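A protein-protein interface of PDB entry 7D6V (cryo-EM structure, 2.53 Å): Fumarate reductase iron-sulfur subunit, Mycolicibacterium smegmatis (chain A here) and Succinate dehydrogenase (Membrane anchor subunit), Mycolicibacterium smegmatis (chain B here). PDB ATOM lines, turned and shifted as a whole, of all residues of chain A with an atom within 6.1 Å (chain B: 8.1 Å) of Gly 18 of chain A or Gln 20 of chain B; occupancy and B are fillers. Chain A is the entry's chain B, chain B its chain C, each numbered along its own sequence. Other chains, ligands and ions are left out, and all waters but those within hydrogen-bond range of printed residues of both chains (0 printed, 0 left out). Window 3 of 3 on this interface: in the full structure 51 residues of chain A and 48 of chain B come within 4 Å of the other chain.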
ATOM      1  N   TRP A  11      -1.332 -15.887  -2.412  1.00  0.00           N
ATOM      2  CA  TRP A  11      -0.183 -15.401  -1.653  1.00  0.00           C
ATOM      3  C   TRP A  11      -0.497 -14.065  -0.983  1.00  0.00           C
ATOM      4  O   TRP A  11      -0.979 -13.134  -1.634  1.00  0.00           O
ATOM      5  CB  TRP A  11       1.029 -15.249  -2.573  1.00  0.00           C
ATOM      6  CG  TRP A  11       2.312 -14.913  -1.861  1.00  0.00           C
ATOM      7  CD1 TRP A  11       3.227 -15.793  -1.372  1.00  0.00           C
ATOM      8  CD2 TRP A  11       2.816 -13.605  -1.559  1.00  0.00           C
ATOM      9  NE1 TRP A  11       4.267 -15.120  -0.785  1.00  0.00           N
ATOM     10  CE2 TRP A  11       4.038 -13.775  -0.884  1.00  0.00           C
ATOM     11  CE3 TRP A  11       2.351 -12.309  -1.789  1.00  0.00           C
ATOM     12  CZ2 TRP A  11       4.800 -12.699  -0.443  1.00  0.00           C
ATOM     13  CZ3 TRP A  11       3.106 -11.246  -1.349  1.00  0.00           C
ATOM     14  CH2 TRP A  11       4.316 -11.445  -0.683  1.00  0.00           C
ATOM     15  N   ARG A  12      -0.215 -13.969   0.316  1.00  0.00           N
ATOM     16  CA  ARG A  12      -0.431 -12.753   1.090  1.00  0.00           C
ATOM     17  C   ARG A  12       0.876 -12.298   1.723  1.00  0.00           C
ATOM     18  O   ARG A  12       1.669 -13.121   2.184  1.00  0.00           O
ATOM     19  CB  ARG A  12      -1.478 -12.961   2.196  1.00  0.00           C
ATOM     20  CG  ARG A  12      -2.774 -13.602   1.754  1.00  0.00           C
ATOM     21  CD  ARG A  12      -3.583 -12.704   0.844  1.00  0.00           C
ATOM     22  NE  ARG A  12      -3.692 -11.337   1.343  1.00  0.00           N
ATOM     23  CZ  ARG A  12      -4.684 -10.891   2.106  1.00  0.00           C
ATOM     24  NH1 ARG A  12      -4.698  -9.630   2.506  1.00  0.00           N
ATOM     25  NH2 ARG A  12      -5.657 -11.707   2.479  1.00  0.00           N
ATOM     26  N   GLY A  13       1.095 -10.994   1.753  1.00  0.00           N
ATOM     27  CA  GLY A  13       2.263 -10.437   2.402  1.00  0.00           C
ATOM     28  C   GLY A  13       2.688  -9.147   1.735  1.00  0.00           C
ATOM     29  O   GLY A  13       1.956  -8.566   0.942  1.00  0.00           O
ATOM     30  N   ASP A  14       3.892  -8.710   2.084  1.00  0.00           N
ATOM     31  CA  ASP A  14       4.489  -7.505   1.513  1.00  0.00           C
ATOM     32  C   ASP A  14       5.984  -7.759   1.346  1.00  0.00           C
ATOM     33  O   ASP A  14       6.453  -8.901   1.394  1.00  0.00           O
ATOM     34  CB  ASP A  14       4.177  -6.265   2.366  1.00  0.00           C
ATOM     35  CG  ASP A  14       4.570  -6.429   3.823  1.00  0.00           C
ATOM     36  OD1 ASP A  14       3.806  -5.969   4.694  1.00  0.00           O
ATOM     37  OD2 ASP A  14       5.636  -7.009   4.104  1.00  0.00           O
ATOM     38  N   THR A  16       8.381  -7.375   3.266  1.00  0.00           N
ATOM     39  CA  THR A  16       9.067  -7.899   4.439  1.00  0.00           C
ATOM     40  C   THR A  16       8.870  -9.396   4.633  1.00  0.00           C
ATOM     41  O   THR A  16       9.449  -9.965   5.563  1.00  0.00           O
ATOM     42  CB  THR A  16       8.607  -7.163   5.702  1.00  0.00           C
ATOM     43  OG1 THR A  16       7.197  -7.347   5.879  1.00  0.00           O
ATOM     44  CG2 THR A  16       8.918  -5.683   5.602  1.00  0.00           C
ATOM     45  N   GLY A  17       8.081 -10.042   3.794  1.00  0.00           N
ATOM     46  CA  GLY A  17       7.812 -11.463   3.915  1.00  0.00           C
ATOM     47  C   GLY A  17       6.375 -11.770   3.545  1.00  0.00           C
ATOM     48  O   GLY A  17       5.513 -10.895   3.484  1.00  0.00           O
ATOM     49  N   GLY A  18       6.110 -13.046   3.300  1.00  0.00           N
ATOM     50  CA  GLY A  18       4.779 -13.428   2.873  1.00  0.00           C
ATOM     51  C   GLY A  18       4.590 -14.925   2.939  1.00  0.00           C
ATOM     52  O   GLY A  18       5.485 -15.671   3.341  1.00  0.00           O
ATOM     53  N   GLU A  19       3.405 -15.354   2.518  1.00  0.00           N
ATOM     54  CA  GLU A  19       2.964 -16.729   2.693  1.00  0.00           C
ATOM     55  C   GLU A  19       1.746 -16.967   1.818  1.00  0.00           C
ATOM     56  O   GLU A  19       1.016 -16.029   1.487  1.00  0.00           O
ATOM     57  CB  GLU A  19       2.626 -17.003   4.162  1.00  0.00           C
ATOM     58  CG  GLU A  19       2.692 -18.446   4.580  1.00  0.00           C
ATOM     59  CD  GLU A  19       2.237 -18.631   6.009  1.00  0.00           C
ATOM     60  OE1 GLU A  19       1.636 -17.688   6.561  1.00  0.00           O
ATOM     61  OE2 GLU A  19       2.474 -19.716   6.579  1.00  0.00           O
ATOM     62  N   LEU A  20       1.532 -18.226   1.452  1.00  0.00           N
ATOM     63  CA  LEU A  20       0.306 -18.618   0.774  1.00  0.00           C
ATOM     64  C   LEU A  20      -0.783 -18.893   1.800  1.00  0.00           C
ATOM     65  O   LEU A  20      -0.516 -19.424   2.881  1.00  0.00           O
ATOM     66  CB  LEU A  20       0.532 -19.857  -0.090  1.00  0.00           C
ATOM     67  CG  LEU A  20       1.519 -19.759  -1.253  1.00  0.00           C
ATOM     68  CD1 LEU A  20       1.853 -21.142  -1.775  1.00  0.00           C
ATOM     69  CD2 LEU A  20       0.975 -18.890  -2.362  1.00  0.00           C
ATOM     70  N   ARG A  93       6.977 -12.697 -10.030  1.00  0.00           N
ATOM     71  CA  ARG A  93       8.159 -13.006  -9.240  1.00  0.00           C
ATOM     72  C   ARG A  93       9.426 -12.341  -9.757  1.00  0.00           C
ATOM     73  O   ARG A  93      10.502 -12.603  -9.219  1.00  0.00           O
ATOM     74  CB  ARG A  93       8.366 -14.521  -9.172  1.00  0.00           C
ATOM     75  CG  ARG A  93       7.377 -15.236  -8.276  1.00  0.00           C
ATOM     76  CD  ARG A  93       7.652 -16.723  -8.228  1.00  0.00           C
ATOM     77  NE  ARG A  93       8.611 -17.066  -7.185  1.00  0.00           N
ATOM     78  CZ  ARG A  93       9.107 -18.283  -6.999  1.00  0.00           C
ATOM     79  NH1 ARG A  93       8.734 -19.277  -7.786  1.00  0.00           N
ATOM     80  NH2 ARG A  93       9.973 -18.508  -6.024  1.00  0.00           N
ATOM     81  N   VAL A  97       7.792  -6.782  -4.814  1.00  0.00           N
ATOM     82  CA  VAL A  97       6.403  -6.944  -4.406  1.00  0.00           C
ATOM     83  C   VAL A  97       5.969  -5.723  -3.605  1.00  0.00           C
ATOM     84  O   VAL A  97       6.659  -5.301  -2.671  1.00  0.00           O
ATOM     85  CB  VAL A  97       6.218  -8.244  -3.603  1.00  0.00           C
ATOM     86  CG1 VAL A  97       7.182  -8.311  -2.431  1.00  0.00           C
ATOM     87  CG2 VAL A  97       4.791  -8.375  -3.119  1.00  0.00           C
ATOM     88  N   VAL B  13      14.839 -15.634  -7.947  1.00  0.00           N
ATOM     89  CA  VAL B  13      13.530 -15.434  -7.342  1.00  0.00           C
ATOM     90  C   VAL B  13      13.595 -15.493  -5.836  1.00  0.00           C
ATOM     91  O   VAL B  13      12.571 -15.296  -5.169  1.00  0.00           O
ATOM     92  CB  VAL B  13      12.494 -16.437  -7.881  1.00  0.00           C
ATOM     93  CG1 VAL B  13      12.257 -16.212  -9.363  1.00  0.00           C
ATOM     94  CG2 VAL B  13      12.957 -17.857  -7.632  1.00  0.00           C
ATOM     95  N   PHE B  14      14.771 -15.759  -5.278  1.00  0.00           N
ATOM     96  CA  PHE B  14      15.011 -15.742  -3.848  1.00  0.00           C
ATOM     97  C   PHE B  14      15.746 -14.482  -3.420  1.00  0.00           C
ATOM     98  O   PHE B  14      16.279 -14.422  -2.309  1.00  0.00           O
ATOM     99  CB  PHE B  14      15.772 -17.003  -3.454  1.00  0.00           C
ATOM    100  CG  PHE B  14      15.279 -18.234  -4.161  1.00  0.00           C
ATOM    101  CD1 PHE B  14      14.055 -18.789  -3.833  1.00  0.00           C
ATOM    102  CD2 PHE B  14      16.019 -18.813  -5.174  1.00  0.00           C
ATOM    103  CE1 PHE B  14      13.590 -19.908  -4.486  1.00  0.00           C
ATOM    104  CE2 PHE B  14      15.559 -19.934  -5.832  1.00  0.00           C
ATOM    105  CZ  PHE B  14      14.343 -20.483  -5.486  1.00  0.00           C
ATOM    106  N   SER B  15      15.779 -13.481  -4.296  1.00  0.00           N
ATOM    107  CA  SER B  15      16.357 -12.188  -4.002  1.00  0.00           C
ATOM    108  C   SER B  15      15.569 -11.494  -2.892  1.00  0.00           C
ATOM    109  O   SER B  15      14.388 -11.783  -2.684  1.00  0.00           O
ATOM    110  CB  SER B  15      16.360 -11.328  -5.261  1.00  0.00           C
ATOM    111  OG  SER B  15      17.138 -11.922  -6.278  1.00  0.00           O
ATOM    112  N   PRO B  16      16.210 -10.582  -2.154  1.00  0.00           N
ATOM    113  CA  PRO B  16      15.547 -10.000  -0.973  1.00  0.00           C
ATOM    114  C   PRO B  16      14.259  -9.248  -1.270  1.00  0.00           C
ATOM    115  O   PRO B  16      13.330  -9.295  -0.456  1.00  0.00           O
ATOM    116  CB  PRO B  16      16.625  -9.068  -0.406  1.00  0.00           C
ATOM    117  CG  PRO B  16      17.903  -9.640  -0.886  1.00  0.00           C
ATOM    118  CD  PRO B  16      17.619 -10.166  -2.251  1.00  0.00           C
ATOM    119  N   ARG B  17      14.167  -8.553  -2.402  1.00  0.00           N
ATOM    120  CA  ARG B  17      13.017  -7.699  -2.676  1.00  0.00           C
ATOM    121  C   ARG B  17      11.857  -8.421  -3.342  1.00  0.00           C
ATOM    122  O   ARG B  17      10.768  -7.846  -3.443  1.00  0.00           O
ATOM    123  CB  ARG B  17      13.427  -6.513  -3.555  1.00  0.00           C
ATOM    124  CG  ARG B  17      14.366  -5.529  -2.894  1.00  0.00           C
ATOM    125  CD  ARG B  17      14.751  -4.430  -3.867  1.00  0.00           C
ATOM    126  NE  ARG B  17      13.595  -3.627  -4.256  1.00  0.00           N
ATOM    127  CZ  ARG B  17      13.159  -2.563  -3.592  1.00  0.00           C
ATOM    128  NH1 ARG B  17      12.097  -1.901  -4.026  1.00  0.00           N
ATOM    129  NH2 ARG B  17      13.779  -2.165  -2.490  1.00  0.00           N
ATOM    130  N   ARG B  18      12.048  -9.650  -3.791  1.00  0.00           N
ATOM    131  CA  ARG B  18      10.999 -10.359  -4.501  1.00  0.00           C
ATOM    132  C   ARG B  18      10.139 -11.154  -3.527  1.00  0.00           C
ATOM    133  O   ARG B  18      10.551 -11.466  -2.408  1.00  0.00           O
ATOM    134  CB  ARG B  18      11.608 -11.265  -5.566  1.00  0.00           C
ATOM    135  CG  ARG B  18      12.560 -10.517  -6.475  1.00  0.00           C
ATOM    136  CD  ARG B  18      12.843 -11.275  -7.740  1.00  0.00           C
ATOM    137  NE  ARG B  18      13.905 -10.660  -8.524  1.00  0.00           N
ATOM    138  CZ  ARG B  18      14.218 -11.029  -9.758  1.00  0.00           C
ATOM    139  NH1 ARG B  18      13.548 -12.007 -10.341  1.00  0.00           N
ATOM    140  NH2 ARG B  18      15.203 -10.427 -10.404  1.00  0.00           N
ATOM    141  N   ALA B  19       8.922 -11.465  -3.966  1.00  0.00           N
ATOM    142  CA  ALA B  19       7.947 -12.101  -3.091  1.00  0.00           C
ATOM    143  C   ALA B  19       8.464 -13.440  -2.580  1.00  0.00           C
ATOM    144  O   ALA B  19       9.079 -14.215  -3.316  1.00  0.00           O
ATOM    145  CB  ALA B  19       6.620 -12.284  -3.822  1.00  0.00           C
ATOM    146  N   GLN B  20       8.208 -13.702  -1.303  1.00  0.00           N
ATOM    147  CA  GLN B  20       8.781 -14.833  -0.578  1.00  0.00           C
ATOM    148  C   GLN B  20       8.043 -16.112  -0.957  1.00  0.00           C
ATOM    149  O   GLN B  20       7.086 -16.525  -0.302  1.00  0.00           O
ATOM    150  CB  GLN B  20       8.717 -14.571   0.921  1.00  0.00           C
ATOM    151  CG  GLN B  20       9.445 -15.574   1.778  1.00  0.00           C
ATOM    152  CD  GLN B  20       9.618 -15.085   3.196  1.00  0.00           C
ATOM    153  OE1 GLN B  20       9.035 -15.630   4.129  1.00  0.00           O
ATOM    154  NE2 GLN B  20      10.417 -14.040   3.366  1.00  0.00           N
ATOM    155  N   ILE B  21       8.496 -16.745  -2.034  1.00  0.00           N
ATOM    156  CA  ILE B  21       8.029 -18.068  -2.439  1.00  0.00           C
ATOM    157  C   ILE B  21       9.219 -19.021  -2.424  1.00  0.00           C
ATOM    158  O   ILE B  21      10.076 -18.949  -3.316  1.00  0.00           O
ATOM    159  CB  ILE B  21       7.346 -18.038  -3.820  1.00  0.00           C
ATOM    160  CG1 ILE B  21       6.083 -17.173  -3.813  1.00  0.00           C
ATOM    161  CG2 ILE B  21       7.025 -19.430  -4.310  1.00  0.00           C
ATOM    162  CD1 ILE B  21       6.298 -15.742  -4.125  1.00  0.00           C
ATOM    163  N   PRO B  22       9.332 -19.921  -1.426  1.00  0.00           N
ATOM    164  CA  PRO B  22      10.477 -20.836  -1.344  1.00  0.00           C
ATOM    165  C   PRO B  22      10.299 -22.109  -2.166  1.00  0.00           C
ATOM    166  O   PRO B  22      10.613 -23.215  -1.716  1.00  0.00           O
ATOM    167  CB  PRO B  22      10.538 -21.152   0.154  1.00  0.00           C
ATOM    168  CG  PRO B  22       9.101 -21.176   0.544  1.00  0.00           C
ATOM    169  CD  PRO B  22       8.404 -20.122  -0.300  1.00  0.00           C
ATOM    170  N   GLU B  23       9.806 -21.962  -3.389  1.00  0.00           N
ATOM    171  CA  GLU B  23       9.643 -23.082  -4.303  1.00  0.00           C
ATOM    172  C   GLU B  23      10.253 -22.720  -5.643  1.00  0.00           C
ATOM    173  O   GLU B  23      10.024 -21.623  -6.159  1.00  0.00           O
ATOM    174  CB  GLU B  23       8.172 -23.489  -4.460  1.00  0.00           C
ATOM    175  CG  GLU B  23       7.559 -24.111  -3.209  1.00  0.00           C
ATOM    176  CD  GLU B  23       6.704 -23.156  -2.403  1.00  0.00           C
ATOM    177  OE1 GLU B  23       6.766 -21.939  -2.649  1.00  0.00           O
ATOM    178  OE2 GLU B  23       5.958 -23.628  -1.522  1.00  0.00           O
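Hydrophobic or aromatic side chains of chain A within 4 Å of the printed part of chain B: Trp 11 and Val 97.
Hydrophobic or aromatic side chains of chain B within 4 Å of the printed part of chain A: Val 13, Ala 19 and Ile 21.
Among the printed residues, 11 pairs touch across the chains.
NE1 of Trp 11 of chain A is in hydrogen-bond range of O of Gln 20 of chain B (3.2 Å).
NH1 of Arg 18 of chain B lies close to O of Arg 93 of chain A (3.3 Å).
NH2 of Arg 93 of chain A is in hydrogen-bond range of O of Ile 21 of chain B.
O of Glu 23 of chain B sits at hydrogen-bond distance from NH2 of Arg 93 of chain A (3.1 Å).
N of Val 97 of chain A lies within hydrogen-bond range of O of Arg 17 of chain B (3.4 Å).
Gly 17 of chain A touches one residue of chain B.
Gly 18 of chain A touches just one residue of chain B: Gln 20 (3.6 Å).
Of the printed residues of chain B, Arg 93 of chain A touches Val 13, Arg 18, Ile 21 and Glu 23.
Of the printed residues of chain A, Val 13 of chain B touches Arg 93.
Of chain A, only Trp 11 (3.2 Å), Gly 17 (3.7 Å) and Gly 18 (3.6 Å) come within 4 Å of Gln 20 of chain B.
Printed residues of chain A within 4 Å of Ile 21 of chain B: Trp 11 and Arg 93.
The nearest residue of chain A that does not touch Gln 20 of chain B is Thr 16 of chain A (4.7 Å).
The nearest printed residue of chain A that does not touch Ala 19 of chain B is Arg 93 of chain A (4.8 Å).
Among the printed residues, pairs that only touch across the chains: Trp 11 of chain A with Ala 19 of chain B (3.9 Å), Trp 11 of chain A with Ile 21 of chain B (3.96 Å), Gly 17 of chain A with Gln 20 of chain B (3.7 Å), Gly 18 of chain A with Gln 20 of chain B (3.6 Å), Arg 93 of chain A with Val 13 of chain B (3.5 Å) and Val 97 of chain A with Ala 19 of chain B (3.9 Å).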
